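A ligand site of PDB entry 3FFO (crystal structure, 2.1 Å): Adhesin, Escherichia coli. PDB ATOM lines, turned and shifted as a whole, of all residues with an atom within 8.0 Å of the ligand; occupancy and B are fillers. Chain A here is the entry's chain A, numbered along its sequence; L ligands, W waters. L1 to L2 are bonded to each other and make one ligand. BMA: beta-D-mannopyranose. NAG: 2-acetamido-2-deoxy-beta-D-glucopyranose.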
ATOM      1  N   ASN A  42     -18.722  -3.981  -4.770  1.00  0.00           N
ATOM      2  CA  ASN A  42     -18.102  -5.304  -4.810  1.00  0.00           C
ATOM      3  C   ASN A  42     -17.129  -5.444  -5.977  1.00  0.00           C
ATOM      4  O   ASN A  42     -17.536  -5.483  -7.135  1.00  0.00           O
ATOM      5  CB  ASN A  42     -19.168  -6.398  -4.892  1.00  0.00           C
ATOM      6  CG  ASN A  42     -18.614  -7.758  -4.497  1.00  0.00           C
ATOM      7  OD1 ASN A  42     -17.405  -7.986  -4.514  1.00  0.00           O
ATOM      8  ND2 ASN A  42     -19.514  -8.669  -4.129  1.00  0.00           N
ATOM      9  N   ALA A  43     -15.846  -5.538  -5.665  1.00  0.00           N
ATOM     10  CA  ALA A  43     -14.829  -5.650  -6.706  1.00  0.00           C
ATOM     11  C   ALA A  43     -14.919  -6.949  -7.513  1.00  0.00           C
ATOM     12  O   ALA A  43     -14.353  -7.032  -8.601  1.00  0.00           O
ATOM     13  CB  ALA A  43     -13.433  -5.477  -6.110  1.00  0.00           C
ATOM     14  N   ASN A  44     -15.628  -7.954  -6.995  1.00  0.00           N
ATOM     15  CA  ASN A  44     -15.585  -9.296  -7.577  1.00  0.00           C
ATOM     16  C   ASN A  44     -16.946  -9.937  -7.829  1.00  0.00           C
ATOM     17  O   ASN A  44     -17.349 -10.843  -7.108  1.00  0.00           O
ATOM     18  CB  ASN A  44     -14.732 -10.211  -6.697  1.00  0.00           C
ATOM     19  CG  ASN A  44     -13.457  -9.536  -6.223  1.00  0.00           C
ATOM     20  OD1 ASN A  44     -12.592  -9.196  -7.027  1.00  0.00           O
ATOM     21  ND2 ASN A  44     -13.349  -9.327  -4.924  1.00  0.00           N
ATOM     22  N   VAL A  45     -17.636  -9.466  -8.854  1.00  0.00           N
ATOM     23  CA  VAL A  45     -18.968  -9.944  -9.183  1.00  0.00           C
ATOM     24  C   VAL A  45     -18.902 -10.967 -10.324  1.00  0.00           C
ATOM     25  O   VAL A  45     -19.728 -11.878 -10.401  1.00  0.00           O
ATOM     26  CB  VAL A  45     -19.907  -8.768  -9.568  1.00  0.00           C
ATOM     27  CG1 VAL A  45     -21.288  -9.274  -9.973  1.00  0.00           C
ATOM     28  CG2 VAL A  45     -20.002  -7.774  -8.419  1.00  0.00           C
ATOM     29  N   TRP A  46     -17.930 -10.782 -11.209  1.00  0.00           N
ATOM     30  CA  TRP A  46     -17.673 -11.734 -12.271  1.00  0.00           C
ATOM     31  C   TRP A  46     -16.165 -11.942 -12.347  1.00  0.00           C
ATOM     32  O   TRP A  46     -15.401 -11.017 -12.096  1.00  0.00           O
ATOM     33  CB  TRP A  46     -18.158 -11.221 -13.626  1.00  0.00           C
ATOM     34  CG  TRP A  46     -19.633 -10.985 -13.727  1.00  0.00           C
ATOM     35  CD1 TRP A  46     -20.582 -11.881 -14.118  1.00  0.00           C
ATOM     36  CD2 TRP A  46     -20.322  -9.762 -13.433  1.00  0.00           C
ATOM     37  NE1 TRP A  46     -21.829 -11.292 -14.084  1.00  0.00           N
ATOM     38  CE2 TRP A  46     -21.692 -10.000 -13.665  1.00  0.00           C
ATOM     39  CE3 TRP A  46     -19.918  -8.498 -12.986  1.00  0.00           C
ATOM     40  CZ2 TRP A  46     -22.671  -9.016 -13.462  1.00  0.00           C
ATOM     41  CZ3 TRP A  46     -20.889  -7.521 -12.792  1.00  0.00           C
ATOM     42  CH2 TRP A  46     -22.251  -7.780 -13.034  1.00  0.00           C
ATOM     43  N   ILE A  48     -13.122 -12.901 -15.002  1.00  0.00           N
ATOM     44  CA  ILE A  48     -12.909 -12.862 -16.448  1.00  0.00           C
ATOM     45  C   ILE A  48     -11.433 -13.069 -16.779  1.00  0.00           C
ATOM     46  O   ILE A  48     -10.567 -12.874 -15.926  1.00  0.00           O
ATOM     47  CB  ILE A  48     -13.401 -11.531 -17.038  1.00  0.00           C
ATOM     48  CG1 ILE A  48     -12.746 -10.346 -16.335  1.00  0.00           C
ATOM     49  CG2 ILE A  48     -14.913 -11.423 -16.912  1.00  0.00           C
ATOM     50  CD1 ILE A  48     -13.133  -9.007 -16.904  1.00  0.00           C
ATOM     51  N   VAL A  54     -15.798  -6.432 -21.223  1.00  0.00           N
ATOM     52  CA  VAL A  54     -17.049  -6.263 -20.527  1.00  0.00           C
ATOM     53  C   VAL A  54     -17.216  -4.850 -19.988  1.00  0.00           C
ATOM     54  O   VAL A  54     -16.261  -4.223 -19.516  1.00  0.00           O
ATOM     55  CB  VAL A  54     -17.156  -7.284 -19.364  1.00  0.00           C
ATOM     56  CG1 VAL A  54     -16.061  -7.012 -18.326  1.00  0.00           C
ATOM     57  CG2 VAL A  54     -18.548  -7.276 -18.754  1.00  0.00           C
ATOM     58  N   LEU A  56     -20.653  -2.318 -18.033  1.00  0.00           N
ATOM     59  CA  LEU A  56     -21.854  -2.438 -17.212  1.00  0.00           C
ATOM     60  C   LEU A  56     -22.982  -1.530 -17.708  1.00  0.00           C
ATOM     61  O   LEU A  56     -22.742  -0.363 -18.012  1.00  0.00           O
ATOM     62  CB  LEU A  56     -21.526  -2.082 -15.770  1.00  0.00           C
ATOM     63  CG  LEU A  56     -20.433  -2.891 -15.067  1.00  0.00           C
ATOM     64  CD1 LEU A  56     -19.993  -2.188 -13.803  1.00  0.00           C
ATOM     65  CD2 LEU A  56     -20.943  -4.284 -14.771  1.00  0.00           C
ATOM     66  N   GLY A  87     -22.204   2.137 -11.447  1.00  0.00           N
ATOM     67  CA  GLY A  87     -21.031   2.031 -12.282  1.00  0.00           C
ATOM     68  C   GLY A  87     -20.032   0.989 -11.850  1.00  0.00           C
ATOM     69  O   GLY A  87     -20.363   0.026 -11.142  1.00  0.00           O
ATOM     70  N   ASP A  88     -18.787   1.193 -12.274  1.00  0.00           N
ATOM     71  CA  ASP A  88     -17.715   0.250 -12.005  1.00  0.00           C
ATOM     72  C   ASP A  88     -17.449   0.211 -10.510  1.00  0.00           C
ATOM     73  O   ASP A  88     -18.036   0.974  -9.765  1.00  0.00           O
ATOM     74  CB  ASP A  88     -16.442   0.675 -12.758  1.00  0.00           C
ATOM     75  CG  ASP A  88     -15.376  -0.416 -12.772  1.00  0.00           C
ATOM     76  OD1 ASP A  88     -15.733  -1.604 -12.640  1.00  0.00           O
ATOM     77  OD2 ASP A  88     -14.189  -0.057 -12.910  1.00  0.00           O
ATOM     78  N   THR A  89     -16.563  -0.675 -10.090  1.00  0.00           N
ATOM     79  CA  THR A  89     -16.325  -0.920  -8.668  1.00  0.00           C
ATOM     80  C   THR A  89     -16.125   0.336  -7.830  1.00  0.00           C
ATOM     81  O   THR A  89     -16.725   0.483  -6.766  1.00  0.00           O
ATOM     82  CB  THR A  89     -15.104  -1.834  -8.465  1.00  0.00           C
ATOM     83  OG1 THR A  89     -15.286  -3.048  -9.200  1.00  0.00           O
ATOM     84  CG2 THR A  89     -14.921  -2.142  -6.999  1.00  0.00           C
ATOM     85  N   ASN A  90     -15.278   1.242  -8.304  1.00  0.00           N
ATOM     86  CA  ASN A  90     -15.010   2.470  -7.580  1.00  0.00           C
ATOM     87  C   ASN A  90     -16.210   3.426  -7.571  1.00  0.00           C
ATOM     88  O   ASN A  90     -16.800   3.712  -8.606  1.00  0.00           O
ATOM     89  CB  ASN A  90     -13.781   3.176  -8.176  1.00  0.00           C
ATOM     90  CG  ASN A  90     -13.357   4.411  -7.375  1.00  0.00           C
ATOM     91  OD1 ASN A  90     -13.663   4.536  -6.190  1.00  0.00           O
ATOM     92  ND2 ASN A  90     -12.661   5.331  -8.045  1.00  0.00           N
ATOM     93  N   ARG A  93     -16.249   6.451  -9.839  1.00  0.00           N
ATOM     94  CA  ARG A  93     -16.523   6.236 -11.255  1.00  0.00           C
ATOM     95  C   ARG A  93     -18.002   6.013 -11.528  1.00  0.00           C
ATOM     96  O   ARG A  93     -18.380   5.627 -12.634  1.00  0.00           O
ATOM     97  CB  ARG A  93     -15.666   5.083 -11.793  1.00  0.00           C
ATOM     98  CG  ARG A  93     -14.318   5.564 -12.317  1.00  0.00           C
ATOM     99  CD  ARG A  93     -13.203   4.564 -12.044  1.00  0.00           C
ATOM    100  NE  ARG A  93     -11.926   5.255 -11.871  1.00  0.00           N
ATOM    101  CZ  ARG A  93     -10.846   4.700 -11.329  1.00  0.00           C
ATOM    102  NH1 ARG A  93      -9.726   5.412 -11.212  1.00  0.00           N
ATOM    103  NH2 ARG A  93     -10.885   3.448 -10.893  1.00  0.00           N
ATOM    104  N   PHE A 106     -20.856   1.895 -17.371  1.00  0.00           N
ATOM    105  CA  PHE A 106     -19.413   1.674 -17.374  1.00  0.00           C
ATOM    106  C   PHE A 106     -19.008   1.259 -18.771  1.00  0.00           C
ATOM    107  O   PHE A 106     -19.426   0.215 -19.279  1.00  0.00           O
ATOM    108  CB  PHE A 106     -19.016   0.603 -16.350  1.00  0.00           C
ATOM    109  CG  PHE A 106     -17.580   0.134 -16.495  1.00  0.00           C
ATOM    110  CD1 PHE A 106     -16.541   1.045 -16.557  1.00  0.00           C
ATOM    111  CD2 PHE A 106     -17.292  -1.224 -16.559  1.00  0.00           C
ATOM    112  CE1 PHE A 106     -15.228   0.626 -16.685  1.00  0.00           C
ATOM    113  CE2 PHE A 106     -15.979  -1.657 -16.677  1.00  0.00           C
ATOM    114  CZ  PHE A 106     -14.941  -0.732 -16.739  1.00  0.00           C
ATOM    115  N   GLY A 108     -16.417   0.092 -20.136  1.00  0.00           N
ATOM    116  CA  GLY A 108     -15.895  -1.259 -20.186  1.00  0.00           C
ATOM    117  C   GLY A 108     -14.378  -1.374 -20.291  1.00  0.00           C
ATOM    118  O   GLY A 108     -13.659  -0.371 -20.346  1.00  0.00           O
ATOM    119  N   TRP A 109     -13.901  -2.612 -20.316  1.00  0.00           N
ATOM    120  CA  TRP A 109     -12.484  -2.904 -20.482  1.00  0.00           C
ATOM    121  C   TRP A 109     -12.301  -4.338 -20.969  1.00  0.00           C
ATOM    122  O   TRP A 109     -13.248  -5.136 -20.968  1.00  0.00           O
ATOM    123  CB  TRP A 109     -11.715  -2.675 -19.176  1.00  0.00           C
ATOM    124  CG  TRP A 109     -11.980  -3.724 -18.140  1.00  0.00           C
ATOM    125  CD1 TRP A 109     -13.195  -4.119 -17.663  1.00  0.00           C
ATOM    126  CD2 TRP A 109     -10.995  -4.498 -17.428  1.00  0.00           C
ATOM    127  NE1 TRP A 109     -13.032  -5.105 -16.714  1.00  0.00           N
ATOM    128  CE2 TRP A 109     -11.699  -5.347 -16.547  1.00  0.00           C
ATOM    129  CE3 TRP A 109      -9.599  -4.542 -17.455  1.00  0.00           C
ATOM    130  CZ2 TRP A 109     -11.041  -6.234 -15.697  1.00  0.00           C
ATOM    131  CZ3 TRP A 109      -8.949  -5.436 -16.606  1.00  0.00           C
ATOM    132  CH2 TRP A 109      -9.679  -6.272 -15.738  1.00  0.00           C
ATOM    133  N   CYS A 110     -11.091  -4.650 -21.409  1.00  0.00           N
ATOM    134  CA  CYS A 110     -10.755  -5.986 -21.870  1.00  0.00           C
ATOM    135  C   CYS A 110      -9.642  -6.562 -21.013  1.00  0.00           C
ATOM    136  O   CYS A 110      -8.600  -5.935 -20.834  1.00  0.00           O
ATOM    137  CB  CYS A 110     -10.327  -5.962 -23.334  1.00  0.00           C
ATOM    138  SG  CYS A 110     -11.641  -5.455 -24.443  1.00  0.00           S
ATOM    139  N   VAL A 111      -9.884  -7.751 -20.478  1.00  0.00           N
ATOM    140  CA  VAL A 111      -8.864  -8.427 -19.701  1.00  0.00           C
ATOM    141  C   VAL A 111      -7.933  -9.126 -20.672  1.00  0.00           C
ATOM    142  O   VAL A 111      -8.382  -9.738 -21.645  1.00  0.00           O
ATOM    143  CB  VAL A 111      -9.491  -9.446 -18.732  1.00  0.00           C
ATOM    144  CG1 VAL A 111     -10.324 -10.461 -19.494  1.00  0.00           C
ATOM    145  CG2 VAL A 111      -8.411 -10.129 -17.909  1.00  0.00           C
ATOM    146  N   TYR A 114      -4.678 -12.827 -18.658  1.00  0.00           N
ATOM    147  CA  TYR A 114      -4.647 -13.120 -17.238  1.00  0.00           C
ATOM    148  C   TYR A 114      -6.077 -13.303 -16.742  1.00  0.00           C
ATOM    149  O   TYR A 114      -7.032 -13.010 -17.473  1.00  0.00           O
ATOM    150  CB  TYR A 114      -3.956 -11.992 -16.470  1.00  0.00           C
ATOM    151  N   LEU A 115      -6.232 -13.801 -15.522  1.00  0.00           N
ATOM    152  CA  LEU A 115      -7.553 -13.850 -14.914  1.00  0.00           C
ATOM    153  C   LEU A 115      -7.684 -12.672 -13.960  1.00  0.00           C
ATOM    154  O   LEU A 115      -6.740 -12.314 -13.249  1.00  0.00           O
ATOM    155  CB  LEU A 115      -7.780 -15.174 -14.177  1.00  0.00           C
ATOM    156  N   SER A 116      -8.861 -12.047 -13.979  1.00  0.00           N
ATOM    157  CA  SER A 116      -9.137 -10.897 -13.140  1.00  0.00           C
ATOM    158  C   SER A 116     -10.631 -10.874 -12.922  1.00  0.00           C
ATOM    159  O   SER A 116     -11.323 -11.848 -13.257  1.00  0.00           O
ATOM    160  CB  SER A 116      -8.680  -9.609 -13.834  1.00  0.00           C
ATOM    161  OG  SER A 116      -8.643  -8.522 -12.933  1.00  0.00           O
ATOM    162  N   THR A 117     -11.147  -9.778 -12.379  1.00  0.00           N
ATOM    163  CA  THR A 117     -12.571  -9.678 -12.083  1.00  0.00           C
ATOM    164  C   THR A 117     -13.208  -8.382 -12.568  1.00  0.00           C
ATOM    165  O   THR A 117     -12.526  -7.371 -12.756  1.00  0.00           O
ATOM    166  CB  THR A 117     -12.839  -9.766 -10.583  1.00  0.00           C
ATOM    167  OG1 THR A 117     -12.038  -8.793  -9.915  1.00  0.00           O
ATOM    168  CG2 THR A 117     -12.511 -11.168 -10.060  1.00  0.00           C
ATOM    169  N   GLN A 118     -14.518  -8.429 -12.753  1.00  0.00           N
ATOM    170  CA  GLN A 118     -15.316  -7.239 -12.993  1.00  0.00           C
ATOM    171  C   GLN A 118     -16.228  -7.021 -11.789  1.00  0.00           C
ATOM    172  O   GLN A 118     -16.948  -7.934 -11.373  1.00  0.00           O
ATOM    173  CB  GLN A 118     -16.168  -7.390 -14.247  1.00  0.00           C
ATOM    174  CG  GLN A 118     -17.092  -6.214 -14.510  1.00  0.00           C
ATOM    175  CD  GLN A 118     -16.320  -4.921 -14.598  1.00  0.00           C
ATOM    176  OE1 GLN A 118     -15.297  -4.836 -15.277  1.00  0.00           O
ATOM    177  NE2 GLN A 118     -16.808  -3.883 -13.912  1.00  0.00           N
ATOM    178  N   GLY A 119     -16.177  -5.814 -11.228  1.00  0.00           N
ATOM    179  CA  GLY A 119     -16.992  -5.476 -10.075  1.00  0.00           C
ATOM    180  C   GLY A 119     -18.013  -4.420 -10.428  1.00  0.00           C
ATOM    181  O   GLY A 119     -18.247  -4.134 -11.608  1.00  0.00           O
ATOM    182  N   LEU A 120     -18.615  -3.828  -9.403  1.00  0.00           N
ATOM    183  CA  LEU A 120     -19.595  -2.758  -9.602  1.00  0.00           C
ATOM    184  C   LEU A 120     -19.847  -2.004  -8.309  1.00  0.00           C
ATOM    185  O   LEU A 120     -19.405  -2.418  -7.229  1.00  0.00           O
ATOM    186  CB  LEU A 120     -20.896  -3.313 -10.159  1.00  0.00           C
ATOM    187  CG  LEU A 120     -21.460  -4.552  -9.466  1.00  0.00           C
ATOM    188  CD1 LEU A 120     -22.108  -4.172  -8.135  1.00  0.00           C
ATOM    189  CD2 LEU A 120     -22.442  -5.276 -10.363  1.00  0.00           C
HETATM  190  C1  BMA L   1      -6.520  -6.216 -11.895  1.00  0.00           C
HETATM  191  C2  BMA L   1      -7.643  -5.434 -12.582  1.00  0.00           C
HETATM  192  C3  BMA L   1      -6.939  -4.556 -13.603  1.00  0.00           C
HETATM  193  C4  BMA L   1      -5.966  -3.619 -12.887  1.00  0.00           C
HETATM  194  C5  BMA L   1      -5.057  -4.372 -11.921  1.00  0.00           C
HETATM  195  C6  BMA L   1      -4.325  -3.400 -11.009  1.00  0.00           C
HETATM  196  O1  BMA L   1      -7.030  -7.263 -11.105  1.00  0.00           O
HETATM  197  O2  BMA L   1      -8.755  -4.805 -11.910  1.00  0.00           O
HETATM  198  O3  BMA L   1      -7.877  -3.824 -14.351  1.00  0.00           O
HETATM  199  O4  BMA L   1      -5.177  -2.932 -13.840  1.00  0.00           O
HETATM  200  O5  BMA L   1      -5.788  -5.285 -11.124  1.00  0.00           O
HETATM  201  O6  BMA L   1      -3.387  -2.657 -11.755  1.00  0.00           O
HETATM  202  C1  NAG L   2     -10.172  -4.873 -12.096  1.00  0.00           C
HETATM  203  C2  NAG L   2     -10.920  -4.819 -10.766  1.00  0.00           C
HETATM  204  C3  NAG L   2     -12.434  -4.872 -10.982  1.00  0.00           C
HETATM  205  C4  NAG L   2     -12.853  -3.823 -11.998  1.00  0.00           C
HETATM  206  C5  NAG L   2     -11.985  -3.863 -13.255  1.00  0.00           C
HETATM  207  C6  NAG L   2     -12.295  -2.680 -14.159  1.00  0.00           C
HETATM  208  C7  NAG L   2      -9.807  -5.723  -8.824  1.00  0.00           C
HETATM  209  C8  NAG L   2      -9.130  -4.402  -8.671  1.00  0.00           C
HETATM  210  N2  NAG L   2     -10.525  -5.925  -9.924  1.00  0.00           N
HETATM  211  O3  NAG L   2     -13.093  -4.670  -9.752  1.00  0.00           O
HETATM  212  O4  NAG L   2     -14.209  -4.018 -12.369  1.00  0.00           O
HETATM  213  O5  NAG L   2     -10.612  -3.810 -12.913  1.00  0.00           O
HETATM  214  O6  NAG L   2     -11.848  -1.508 -13.507  1.00  0.00           O
HETATM  215  O7  NAG L   2      -9.691  -6.581  -7.959  1.00  0.00           O
HETATM  216  O   HOH W   1      -5.591  -6.134  -8.421  1.00  0.00           O
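O1 of BMA L1 sits at hydrogen-bond distance from OG of Ser 116.
OG1 of Thr 89 is in hydrogen-bond range of O3 of NAG L2, 2.8 Å away.
The side-chain carboxylate (OD2) of Asp 88 sits at hydrogen-bond distance from an oxygen (O6) of NAG L2 (2.8 Å).
The backbone NH (N) of Gly 119 sits at hydrogen-bond distance from an oxygen (O4) of NAG L2, at 2.9 Å.
O of Ala 43 is in hydrogen-bond range of O3 of NAG L2 (2.9 Å).
The side-chain amide nitrogen (NE2) of Gln 118 is in hydrogen-bond range of an oxygen (O4) of NAG L2 (3.0 Å).
The side-chain hydroxyl of Thr 117 lies within hydrogen-bond range of a nitrogen (N2) of NAG L2 (3.2 Å).
CZ3 of Trp 109 touches O3 of BMA L1, 3.0 Å away.
Hydrophobic or aromatic side chains within 4 Å of the ligand: Ala 43 and Trp 109.
Eight residues have an atom within 4 Å of the ligand: Ala 43, Asp 88, Thr 89, Trp 109, Ser 116, Thr 117, Gln 118 and Gly 119.
Along chain A the residues within 4 Å of the ligand span positions 43 to 119.
O of Ile 48 is in hydrogen-bond range of N of Ser 116, at 2.7 Å.
The side-chain hydroxyl (OG1) of Thr 89 is in hydrogen-bond range of the backbone NH (N) of Leu 120 (3.4 Å).
The backbone NH of Gly 119 lies close to the backbone carbonyl oxygen of Ala 43.
The backbone carbonyl oxygen (O) of Ala 43 sits at hydrogen-bond distance from the side-chain hydroxyl (OG1) of Thr 117 (3.2 Å).
NE1 of Trp 109 lies within hydrogen-bond range of OE1 of Gln 118 (2.7 Å).
The backbone NH (N) of Val 54 sits at hydrogen-bond distance from the backbone carbonyl oxygen (O) of Trp 109 (2.9 Å).
The backbone NH (N) of Gln 118 is in hydrogen-bond range of the backbone carbonyl oxygen (O) of Trp 46 (2.8 Å).
OD1 of Asn 44 lies within hydrogen-bond range of OG1 of Thr 117.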
